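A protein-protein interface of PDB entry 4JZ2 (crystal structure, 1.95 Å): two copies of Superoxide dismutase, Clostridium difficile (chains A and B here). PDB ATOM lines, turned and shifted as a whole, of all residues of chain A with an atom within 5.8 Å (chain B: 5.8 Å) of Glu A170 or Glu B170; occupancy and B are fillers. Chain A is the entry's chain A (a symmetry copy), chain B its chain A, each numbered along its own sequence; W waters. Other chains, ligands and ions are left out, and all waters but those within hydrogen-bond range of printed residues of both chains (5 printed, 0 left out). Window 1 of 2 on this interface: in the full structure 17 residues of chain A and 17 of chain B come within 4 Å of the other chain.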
ATOM      1  N   HIS A  34      28.968  -5.610  -6.786  1.00  0.00           N
ATOM      2  CA  HIS A  34      29.737  -6.852  -6.644  1.00  0.00           C
ATOM      3  C   HIS A  34      31.238  -6.655  -6.849  1.00  0.00           C
ATOM      4  O   HIS A  34      32.042  -7.022  -5.998  1.00  0.00           O
ATOM      5  CB  HIS A  34      29.219  -7.927  -7.594  1.00  0.00           C
ATOM      6  CG  HIS A  34      27.828  -8.381  -7.286  1.00  0.00           C
ATOM      7  ND1 HIS A  34      27.556  -9.401  -6.395  1.00  0.00           N
ATOM      8  CD2 HIS A  34      26.623  -7.959  -7.747  1.00  0.00           C
ATOM      9  CE1 HIS A  34      26.247  -9.583  -6.323  1.00  0.00           C
ATOM     10  NE2 HIS A  34      25.661  -8.722  -7.141  1.00  0.00           N
ATOM     11  N   SER A 131      28.377 -21.546  -7.989  1.00  0.00           N
ATOM     12  CA  SER A 131      28.920 -20.300  -8.537  1.00  0.00           C
ATOM     13  C   SER A 131      30.259 -20.586  -9.228  1.00  0.00           C
ATOM     14  O   SER A 131      31.009 -21.450  -8.787  1.00  0.00           O
ATOM     15  CB  SER A 131      29.133 -19.271  -7.419  1.00  0.00           C
ATOM     16  OG  SER A 131      27.941 -19.078  -6.654  1.00  0.00           O
ATOM     17  N   VAL A 168      29.341 -17.169 -14.491  1.00  0.00           N
ATOM     18  CA  VAL A 168      28.041 -17.850 -14.350  1.00  0.00           C
ATOM     19  C   VAL A 168      27.530 -17.915 -12.914  1.00  0.00           C
ATOM     20  O   VAL A 168      26.673 -18.746 -12.583  1.00  0.00           O
ATOM     21  CB  VAL A 168      27.972 -19.249 -15.027  1.00  0.00           C
ATOM     22  CG1 VAL A 168      28.121 -19.107 -16.539  1.00  0.00           C
ATOM     23  CG2 VAL A 168      29.021 -20.196 -14.432  1.00  0.00           C
ATOM     24  N   TRP A 169      28.052 -17.036 -12.065  1.00  0.00           N
ATOM     25  CA  TRP A 169      27.389 -16.746 -10.799  1.00  0.00           C
ATOM     26  C   TRP A 169      25.980 -16.296 -11.180  1.00  0.00           C
ATOM     27  O   TRP A 169      25.799 -15.613 -12.196  1.00  0.00           O
ATOM     28  CB  TRP A 169      28.092 -15.605 -10.087  1.00  0.00           C
ATOM     29  CG  TRP A 169      29.370 -16.005  -9.364  1.00  0.00           C
ATOM     30  CD1 TRP A 169      30.483 -16.596  -9.912  1.00  0.00           C
ATOM     31  CD2 TRP A 169      29.651 -15.829  -7.975  1.00  0.00           C
ATOM     32  NE1 TRP A 169      31.445 -16.794  -8.935  1.00  0.00           N
ATOM     33  CE2 TRP A 169      30.951 -16.326  -7.733  1.00  0.00           C
ATOM     34  CE3 TRP A 169      28.929 -15.287  -6.896  1.00  0.00           C
ATOM     35  CZ2 TRP A 169      31.541 -16.306  -6.471  1.00  0.00           C
ATOM     36  CZ3 TRP A 169      29.517 -15.265  -5.640  1.00  0.00           C
ATOM     37  CH2 TRP A 169      30.812 -15.775  -5.436  1.00  0.00           C
ATOM     38  N   GLU A 170      24.988 -16.653 -10.370  1.00  0.00           N
ATOM     39  CA  GLU A 170      23.606 -16.263 -10.663  1.00  0.00           C
ATOM     40  C   GLU A 170      23.411 -14.740 -10.672  1.00  0.00           C
ATOM     41  O   GLU A 170      22.527 -14.233 -11.364  1.00  0.00           O
ATOM     42  CB  GLU A 170      22.629 -16.963  -9.693  1.00  0.00           C
ATOM     43  CG  GLU A 170      22.539 -18.474  -9.975  1.00  0.00           C
ATOM     44  CD  GLU A 170      21.790 -19.281  -8.908  1.00  0.00           C
ATOM     45  OE1 GLU A 170      21.885 -18.955  -7.703  1.00  0.00           O
ATOM     46  OE2 GLU A 170      21.130 -20.268  -9.286  1.00  0.00           O
ATOM     47  N   HIS A 171      24.217 -13.998  -9.918  1.00  0.00           N
ATOM     48  CA  HIS A 171      24.063 -12.542  -9.969  1.00  0.00           C
ATOM     49  C   HIS A 171      24.336 -11.949 -11.365  1.00  0.00           C
ATOM     50  O   HIS A 171      23.850 -10.855 -11.695  1.00  0.00           O
ATOM     51  CB  HIS A 171      24.879 -11.827  -8.891  1.00  0.00           C
ATOM     52  CG  HIS A 171      26.369 -11.940  -9.061  1.00  0.00           C
ATOM     53  ND1 HIS A 171      27.196 -12.425  -8.072  1.00  0.00           N
ATOM     54  CD2 HIS A 171      27.173 -11.598 -10.097  1.00  0.00           C
ATOM     55  CE1 HIS A 171      28.449 -12.394  -8.498  1.00  0.00           C
ATOM     56  NE2 HIS A 171      28.462 -11.884  -9.717  1.00  0.00           N
ATOM     57  N   ALA A 172      25.102 -12.669 -12.176  1.00  0.00           N
ATOM     58  CA  ALA A 172      25.444 -12.214 -13.524  1.00  0.00           C
ATOM     59  C   ALA A 172      24.277 -12.307 -14.499  1.00  0.00           C
ATOM     60  O   ALA A 172      24.297 -11.656 -15.548  1.00  0.00           O
ATOM     61  CB  ALA A 172      26.619 -13.019 -14.083  1.00  0.00           C
ATOM     62  N   TYR A 173      23.277 -13.124 -14.182  1.00  0.00           N
ATOM     63  CA  TYR A 173      22.203 -13.353 -15.145  1.00  0.00           C
ATOM     64  C   TYR A 173      20.772 -13.462 -14.602  1.00  0.00           C
ATOM     65  O   TYR A 173      19.827 -13.552 -15.388  1.00  0.00           O
ATOM     66  CB  TYR A 173      22.511 -14.603 -15.979  1.00  0.00           C
ATOM     67  CG  TYR A 173      22.548 -15.926 -15.220  1.00  0.00           C
ATOM     68  CD1 TYR A 173      21.379 -16.647 -14.967  1.00  0.00           C
ATOM     69  CD2 TYR A 173      23.757 -16.473 -14.796  1.00  0.00           C
ATOM     70  CE1 TYR A 173      21.421 -17.892 -14.301  1.00  0.00           C
ATOM     71  CE2 TYR A 173      23.806 -17.704 -14.131  1.00  0.00           C
ATOM     72  CZ  TYR A 173      22.641 -18.401 -13.885  1.00  0.00           C
ATOM     73  OH  TYR A 173      22.705 -19.617 -13.223  1.00  0.00           O
ATOM     74  N   TYR A 174      20.594 -13.473 -13.285  1.00  0.00           N
ATOM     75  CA  TYR A 174      19.259 -13.783 -12.757  1.00  0.00           C
ATOM     76  C   TYR A 174      18.175 -12.739 -13.088  1.00  0.00           C
ATOM     77  O   TYR A 174      17.044 -13.105 -13.398  1.00  0.00           O
ATOM     78  CB  TYR A 174      19.270 -14.086 -11.253  1.00  0.00           C
ATOM     79  CG  TYR A 174      18.289 -15.191 -10.925  1.00  0.00           C
ATOM     80  CD1 TYR A 174      18.577 -16.518 -11.238  1.00  0.00           C
ATOM     81  CD2 TYR A 174      17.055 -14.909 -10.353  1.00  0.00           C
ATOM     82  CE1 TYR A 174      17.667 -17.540 -10.969  1.00  0.00           C
ATOM     83  CE2 TYR A 174      16.141 -15.929 -10.064  1.00  0.00           C
ATOM     84  CZ  TYR A 174      16.446 -17.231 -10.377  1.00  0.00           C
ATOM     85  OH  TYR A 174      15.526 -18.226 -10.102  1.00  0.00           O
ATOM     86  N   LEU A 175      18.513 -11.456 -13.008  1.00  0.00           N
ATOM     87  CA  LEU A 175      17.515 -10.406 -13.256  1.00  0.00           C
ATOM     88  C   LEU A 175      16.851 -10.564 -14.624  1.00  0.00           C
ATOM     89  O   LEU A 175      15.638 -10.427 -14.757  1.00  0.00           O
ATOM     90  CB  LEU A 175      18.111  -8.999 -13.087  1.00  0.00           C
ATOM     91  CG  LEU A 175      18.503  -8.598 -11.664  1.00  0.00           C
ATOM     92  CD1 LEU A 175      18.833  -7.123 -11.601  1.00  0.00           C
ATOM     93  CD2 LEU A 175      17.393  -8.938 -10.653  1.00  0.00           C
ATOM     94  N   ARG A 181      20.012 -20.221 -17.533  1.00  0.00           N
ATOM     95  CA  ARG A 181      21.409 -19.882 -17.763  1.00  0.00           C
ATOM     96  C   ARG A 181      21.787 -20.167 -19.210  1.00  0.00           C
ATOM     97  O   ARG A 181      22.591 -19.441 -19.803  1.00  0.00           O
ATOM     98  CB  ARG A 181      22.339 -20.646 -16.807  1.00  0.00           C
ATOM     99  CG  ARG A 181      23.795 -20.146 -16.845  1.00  0.00           C
ATOM    100  CD  ARG A 181      24.766 -21.188 -16.252  1.00  0.00           C
ATOM    101  NE  ARG A 181      24.603 -21.356 -14.803  1.00  0.00           N
ATOM    102  CZ  ARG A 181      25.299 -22.242 -14.085  1.00  0.00           C
ATOM    103  NH1 ARG A 181      26.193 -23.037 -14.679  1.00  0.00           N
ATOM    104  NH2 ARG A 181      25.109 -22.346 -12.778  1.00  0.00           N
ATOM    105  N   HIS B  34      13.906 -24.506 -10.064  1.00  0.00           N
ATOM    106  CA  HIS B  34      15.135 -24.992  -9.424  1.00  0.00           C
ATOM    107  C   HIS B  34      14.948 -26.327  -8.705  1.00  0.00           C
ATOM    108  O   HIS B  34      15.675 -27.283  -8.957  1.00  0.00           O
ATOM    109  CB  HIS B  34      15.695 -23.954  -8.458  1.00  0.00           C
ATOM    110  CG  HIS B  34      16.162 -22.701  -9.128  1.00  0.00           C
ATOM    111  ND1 HIS B  34      17.443 -22.553  -9.624  1.00  0.00           N
ATOM    112  CD2 HIS B  34      15.526 -21.530  -9.387  1.00  0.00           C
ATOM    113  CE1 HIS B  34      17.571 -21.350 -10.159  1.00  0.00           C
ATOM    114  NE2 HIS B  34      16.420 -20.708 -10.021  1.00  0.00           N
ATOM    115  N   SER B 131      27.879 -20.145  -3.623  1.00  0.00           N
ATOM    116  CA  SER B 131      26.548 -20.709  -3.384  1.00  0.00           C
ATOM    117  C   SER B 131      26.593 -21.621  -2.151  1.00  0.00           C
ATOM    118  O   SER B 131      27.600 -22.276  -1.904  1.00  0.00           O
ATOM    119  CB  SER B 131      26.084 -21.521  -4.600  1.00  0.00           C
ATOM    120  OG  SER B 131      26.160 -20.749  -5.802  1.00  0.00           O
ATOM    121  N   VAL B 168      21.270 -19.639   0.668  1.00  0.00           N
ATOM    122  CA  VAL B 168      21.881 -18.362   0.258  1.00  0.00           C
ATOM    123  C   VAL B 168      22.504 -18.394  -1.134  1.00  0.00           C
ATOM    124  O   VAL B 168      23.352 -17.555  -1.469  1.00  0.00           O
ATOM    125  CB  VAL B 168      22.871 -17.760   1.295  1.00  0.00           C
ATOM    126  CG1 VAL B 168      22.127 -17.387   2.575  1.00  0.00           C
ATOM    127  CG2 VAL B 168      24.031 -18.724   1.565  1.00  0.00           C
ATOM    128  N   TRP B 169      22.081 -19.359  -1.944  1.00  0.00           N
ATOM    129  CA  TRP B 169      22.303 -19.268  -3.382  1.00  0.00           C
ATOM    130  C   TRP B 169      21.664 -17.946  -3.803  1.00  0.00           C
ATOM    131  O   TRP B 169      20.616 -17.566  -3.269  1.00  0.00           O
ATOM    132  CB  TRP B 169      21.596 -20.404  -4.096  1.00  0.00           C
ATOM    133  CG  TRP B 169      22.323 -21.739  -4.034  1.00  0.00           C
ATOM    134  CD1 TRP B 169      22.694 -22.431  -2.907  1.00  0.00           C
ATOM    135  CD2 TRP B 169      22.750 -22.528  -5.146  1.00  0.00           C
ATOM    136  NE1 TRP B 169      23.326 -23.613  -3.259  1.00  0.00           N
ATOM    137  CE2 TRP B 169      23.369 -23.691  -4.638  1.00  0.00           C
ATOM    138  CE3 TRP B 169      22.663 -22.370  -6.541  1.00  0.00           C
ATOM    139  CZ2 TRP B 169      23.902 -24.681  -5.460  1.00  0.00           C
ATOM    140  CZ3 TRP B 169      23.191 -23.357  -7.362  1.00  0.00           C
ATOM    141  CH2 TRP B 169      23.806 -24.500  -6.818  1.00  0.00           C
ATOM    142  N   GLU B 170      22.272 -17.257  -4.764  1.00  0.00           N
ATOM    143  CA  GLU B 170      21.725 -15.978  -5.226  1.00  0.00           C
ATOM    144  C   GLU B 170      20.325 -16.122  -5.841  1.00  0.00           C
ATOM    145  O   GLU B 170      19.533 -15.179  -5.805  1.00  0.00           O
ATOM    146  CB  GLU B 170      22.710 -15.285  -6.192  1.00  0.00           C
ATOM    147  CG  GLU B 170      23.964 -14.781  -5.455  1.00  0.00           C
ATOM    148  CD  GLU B 170      25.098 -14.308  -6.371  1.00  0.00           C
ATOM    149  OE1 GLU B 170      25.303 -14.893  -7.460  1.00  0.00           O
ATOM    150  OE2 GLU B 170      25.807 -13.362  -5.975  1.00  0.00           O
ATOM    151  N   HIS B 171      20.002 -17.282  -6.407  1.00  0.00           N
ATOM    152  CA  HIS B 171      18.649 -17.433  -6.945  1.00  0.00           C
ATOM    153  C   HIS B 171      17.549 -17.311  -5.873  1.00  0.00           C
ATOM    154  O   HIS B 171      16.392 -16.985  -6.186  1.00  0.00           O
ATOM    155  CB  HIS B 171      18.484 -18.712  -7.769  1.00  0.00           C
ATOM    156  CG  HIS B 171      18.594 -19.983  -6.972  1.00  0.00           C
ATOM    157  ND1 HIS B 171      19.486 -20.984  -7.288  1.00  0.00           N
ATOM    158  CD2 HIS B 171      17.898 -20.418  -5.895  1.00  0.00           C
ATOM    159  CE1 HIS B 171      19.347 -21.980  -6.427  1.00  0.00           C
ATOM    160  NE2 HIS B 171      18.382 -21.666  -5.580  1.00  0.00           N
ATOM    161  N   ALA B 172      17.909 -17.566  -4.621  1.00  0.00           N
ATOM    162  CA  ALA B 172      16.958 -17.494  -3.511  1.00  0.00           C
ATOM    163  C   ALA B 172      16.580 -16.065  -3.142  1.00  0.00           C
ATOM    164  O   ALA B 172      15.557 -15.848  -2.485  1.00  0.00           O
ATOM    165  CB  ALA B 172      17.521 -18.192  -2.272  1.00  0.00           C
ATOM    166  N   TYR B 173      17.402 -15.094  -3.528  1.00  0.00           N
ATOM    167  CA  TYR B 173      17.159 -13.725  -3.081  1.00  0.00           C
ATOM    168  C   TYR B 173      17.407 -12.593  -4.086  1.00  0.00           C
ATOM    169  O   TYR B 173      17.117 -11.435  -3.784  1.00  0.00           O
ATOM    170  CB  TYR B 173      17.969 -13.442  -1.809  1.00  0.00           C
ATOM    171  CG  TYR B 173      19.487 -13.464  -1.960  1.00  0.00           C
ATOM    172  CD1 TYR B 173      20.187 -12.337  -2.396  1.00  0.00           C
ATOM    173  CD2 TYR B 173      20.222 -14.598  -1.623  1.00  0.00           C
ATOM    174  CE1 TYR B 173      21.595 -12.347  -2.494  1.00  0.00           C
ATOM    175  CE2 TYR B 173      21.618 -14.618  -1.721  1.00  0.00           C
ATOM    176  CZ  TYR B 173      22.293 -13.497  -2.160  1.00  0.00           C
ATOM    177  OH  TYR B 173      23.675 -13.531  -2.255  1.00  0.00           O
ATOM    178  N   TYR B 174      17.950 -12.898  -5.260  1.00  0.00           N
ATOM    179  CA  TYR B 174      18.380 -11.805  -6.143  1.00  0.00           C
ATOM    180  C   TYR B 174      17.238 -10.923  -6.683  1.00  0.00           C
ATOM    181  O   TYR B 174      17.385  -9.707  -6.758  1.00  0.00           O
ATOM    182  CB  TYR B 174      19.276 -12.286  -7.292  1.00  0.00           C
ATOM    183  CG  TYR B 174      20.366 -11.276  -7.577  1.00  0.00           C
ATOM    184  CD1 TYR B 174      21.459 -11.143  -6.724  1.00  0.00           C
ATOM    185  CD2 TYR B 174      20.281 -10.417  -8.666  1.00  0.00           C
ATOM    186  CE1 TYR B 174      22.453 -10.194  -6.960  1.00  0.00           C
ATOM    187  CE2 TYR B 174      21.280  -9.470  -8.922  1.00  0.00           C
ATOM    188  CZ  TYR B 174      22.352  -9.359  -8.070  1.00  0.00           C
ATOM    189  OH  TYR B 174      23.323  -8.408  -8.325  1.00  0.00           O
ATOM    190  N   LEU B 175      16.121 -11.533  -7.068  1.00  0.00           N
ATOM    191  CA  LEU B 175      15.013 -10.760  -7.645  1.00  0.00           C
ATOM    192  C   LEU B 175      14.558  -9.635  -6.714  1.00  0.00           C
ATOM    193  O   LEU B 175      14.316  -8.514  -7.151  1.00  0.00           O
ATOM    194  CB  LEU B 175      13.833 -11.662  -8.043  1.00  0.00           C
ATOM    195  CG  LEU B 175      14.074 -12.611  -9.217  1.00  0.00           C
ATOM    196  CD1 LEU B 175      12.775 -13.248  -9.660  1.00  0.00           C
ATOM    197  CD2 LEU B 175      14.742 -11.889 -10.402  1.00  0.00           C
ATOM    198  N   ARG B 181      22.310  -9.418   0.466  1.00  0.00           N
ATOM    199  CA  ARG B 181      21.980 -10.680   1.114  1.00  0.00           C
ATOM    200  C   ARG B 181      21.663 -10.448   2.585  1.00  0.00           C
ATOM    201  O   ARG B 181      20.800 -11.122   3.154  1.00  0.00           O
ATOM    202  CB  ARG B 181      23.116 -11.703   0.967  1.00  0.00           C
ATOM    203  CG  ARG B 181      22.722 -13.121   1.420  1.00  0.00           C
ATOM    204  CD  ARG B 181      23.965 -13.993   1.694  1.00  0.00           C
ATOM    205  NE  ARG B 181      24.705 -14.326   0.471  1.00  0.00           N
ATOM    206  CZ  ARG B 181      25.843 -15.026   0.472  1.00  0.00           C
ATOM    207  NH1 ARG B 181      26.368 -15.458   1.620  1.00  0.00           N
ATOM    208  NH2 ARG B 181      26.466 -15.295  -0.667  1.00  0.00           N
HETATM  209  O   HOH W   1      24.184 -18.917  -6.374  1.00  0.00           O
HETATM  210  O   HOH W   2      24.559  -8.223 -10.903  1.00  0.00           O
HETATM  211  O   HOH W   3      14.360 -18.473  -7.496  1.00  0.00           O
HETATM  212  O   HOH W   4      29.420 -21.963  -5.301  1.00  0.00           O
HETATM  213  O   HOH W   5      25.935 -17.465  -7.641  1.00  0.00           O
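Among the printed residues, merely in contact across the chains: His A171 with Tyr B174, Tyr A174 with His B171, Glu A170 with Trp B169, Trp A169 with Glu B170, Tyr A174 with Leu B175, Leu A175 with Tyr B174, His A34 with Glu B170, Glu A170 with His B34 and Leu A175 with Leu B175.
His A34 touches Tyr B174, and with the chains exchanged Tyr A174 touches His B34. Glu A170 touches its own counterpart, Glu B170. His A171 touches Tyr B174, and with the chains exchanged Tyr A174 touches His B171. Leu B175 touches its own counterpart, Leu A175. 11 positions are printed for both chains. Of the 15 pairs that touch across the chains among the printed residues, 15 have their exchanged pair printed and touching as well.
Water W5 lies within hydrogen-bond range of the side-chain carboxylate (OE1) of Glu B170 (2.7 Å), the side-chain hydroxyl (OG) of Ser A131 (2.8 Å) and the backbone NH (N) of Glu A170 (3.0 Å). Water W1 lies within hydrogen-bond range of the side-chain carboxylate (OE1) of Glu A170 (2.7 Å), the side-chain hydroxyl (OG) of Ser B131 (2.8 Å) and the backbone NH (N) of Glu B170 (3.0 Å). Water W2 lies within hydrogen-bond range of O of His A171 (2.8 Å) and OH of Tyr B174 (2.9 Å). Water W3 lies within hydrogen-bond range of O of His B171 (2.8 Å) and OH of Tyr A174 (2.9 Å). Water W4 lies within hydrogen-bond range of the backbone NH of Ser A131 and the backbone NH of Ser B131.
Of the 11 printed residues of chain A, 7 touch a printed residue of chain B. Of the 11 printed residues of chain B, 7 touch a printed residue of chain A. Along chain B the printed residues that touch a printed residue of chain A span positions 34 to 175. Among the printed residues, 15 pairs touch across the chains. Among the printed residues, no Asp or Glu carboxylate lies within 4 Å of a Lys or Arg side-chain nitrogen of the other chain.
ND1 of His B171 sits close to ND1 of His B34 (3.5 Å). ND1 of His A34 sits close to ND1 of His A171, 3.5 Å away.
The side-chain hydroxyl (OH) of Tyr A174 sits at hydrogen-bond distance from a ring nitrogen (NE2) of His B34, 2.6 Å away. The side-chain hydroxyl of Ser A131 sits at hydrogen-bond distance from the side-chain hydroxyl of Ser B131 (2.6 Å). OE1 of Glu B170 lies within hydrogen-bond range of N of Glu A170 (3.4 Å). The side-chain carboxylate (OE2) of Glu B170 lies within hydrogen-bond range of a ring nitrogen (ND1) of His A171 (2.7 Å). The side-chain carboxylate (OE2) of Glu A170 sits at hydrogen-bond distance from a ring nitrogen (ND1) of His B171, at 2.7 Å. OH of Tyr B174 lies within hydrogen-bond range of NE2 of His A34 (2.6 Å).
Of chain B, only His B34, Trp B169, Glu B170 and His B171 come within 4 Å of Glu A170. Glu B170 touches just these residues of chain A: His A34, Trp A169, Glu A170 and His A171. Printed residues of chain A within 4 Å of Ser B131: Ser A131. Printed residues of chain A within 4 Å of Trp B169: Glu A170. Val B168 touches none of the printed residues of chain A. The nearest residue of chain B that does not touch Glu A170 is Ser B131 (5.0 Å). The nearest residue of chain A that does not touch Glu B170 is Ser A131 (5.0 Å). The nearest printed residue of chain B that does not touch Ser A131 is Glu B170 (5.0 Å).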
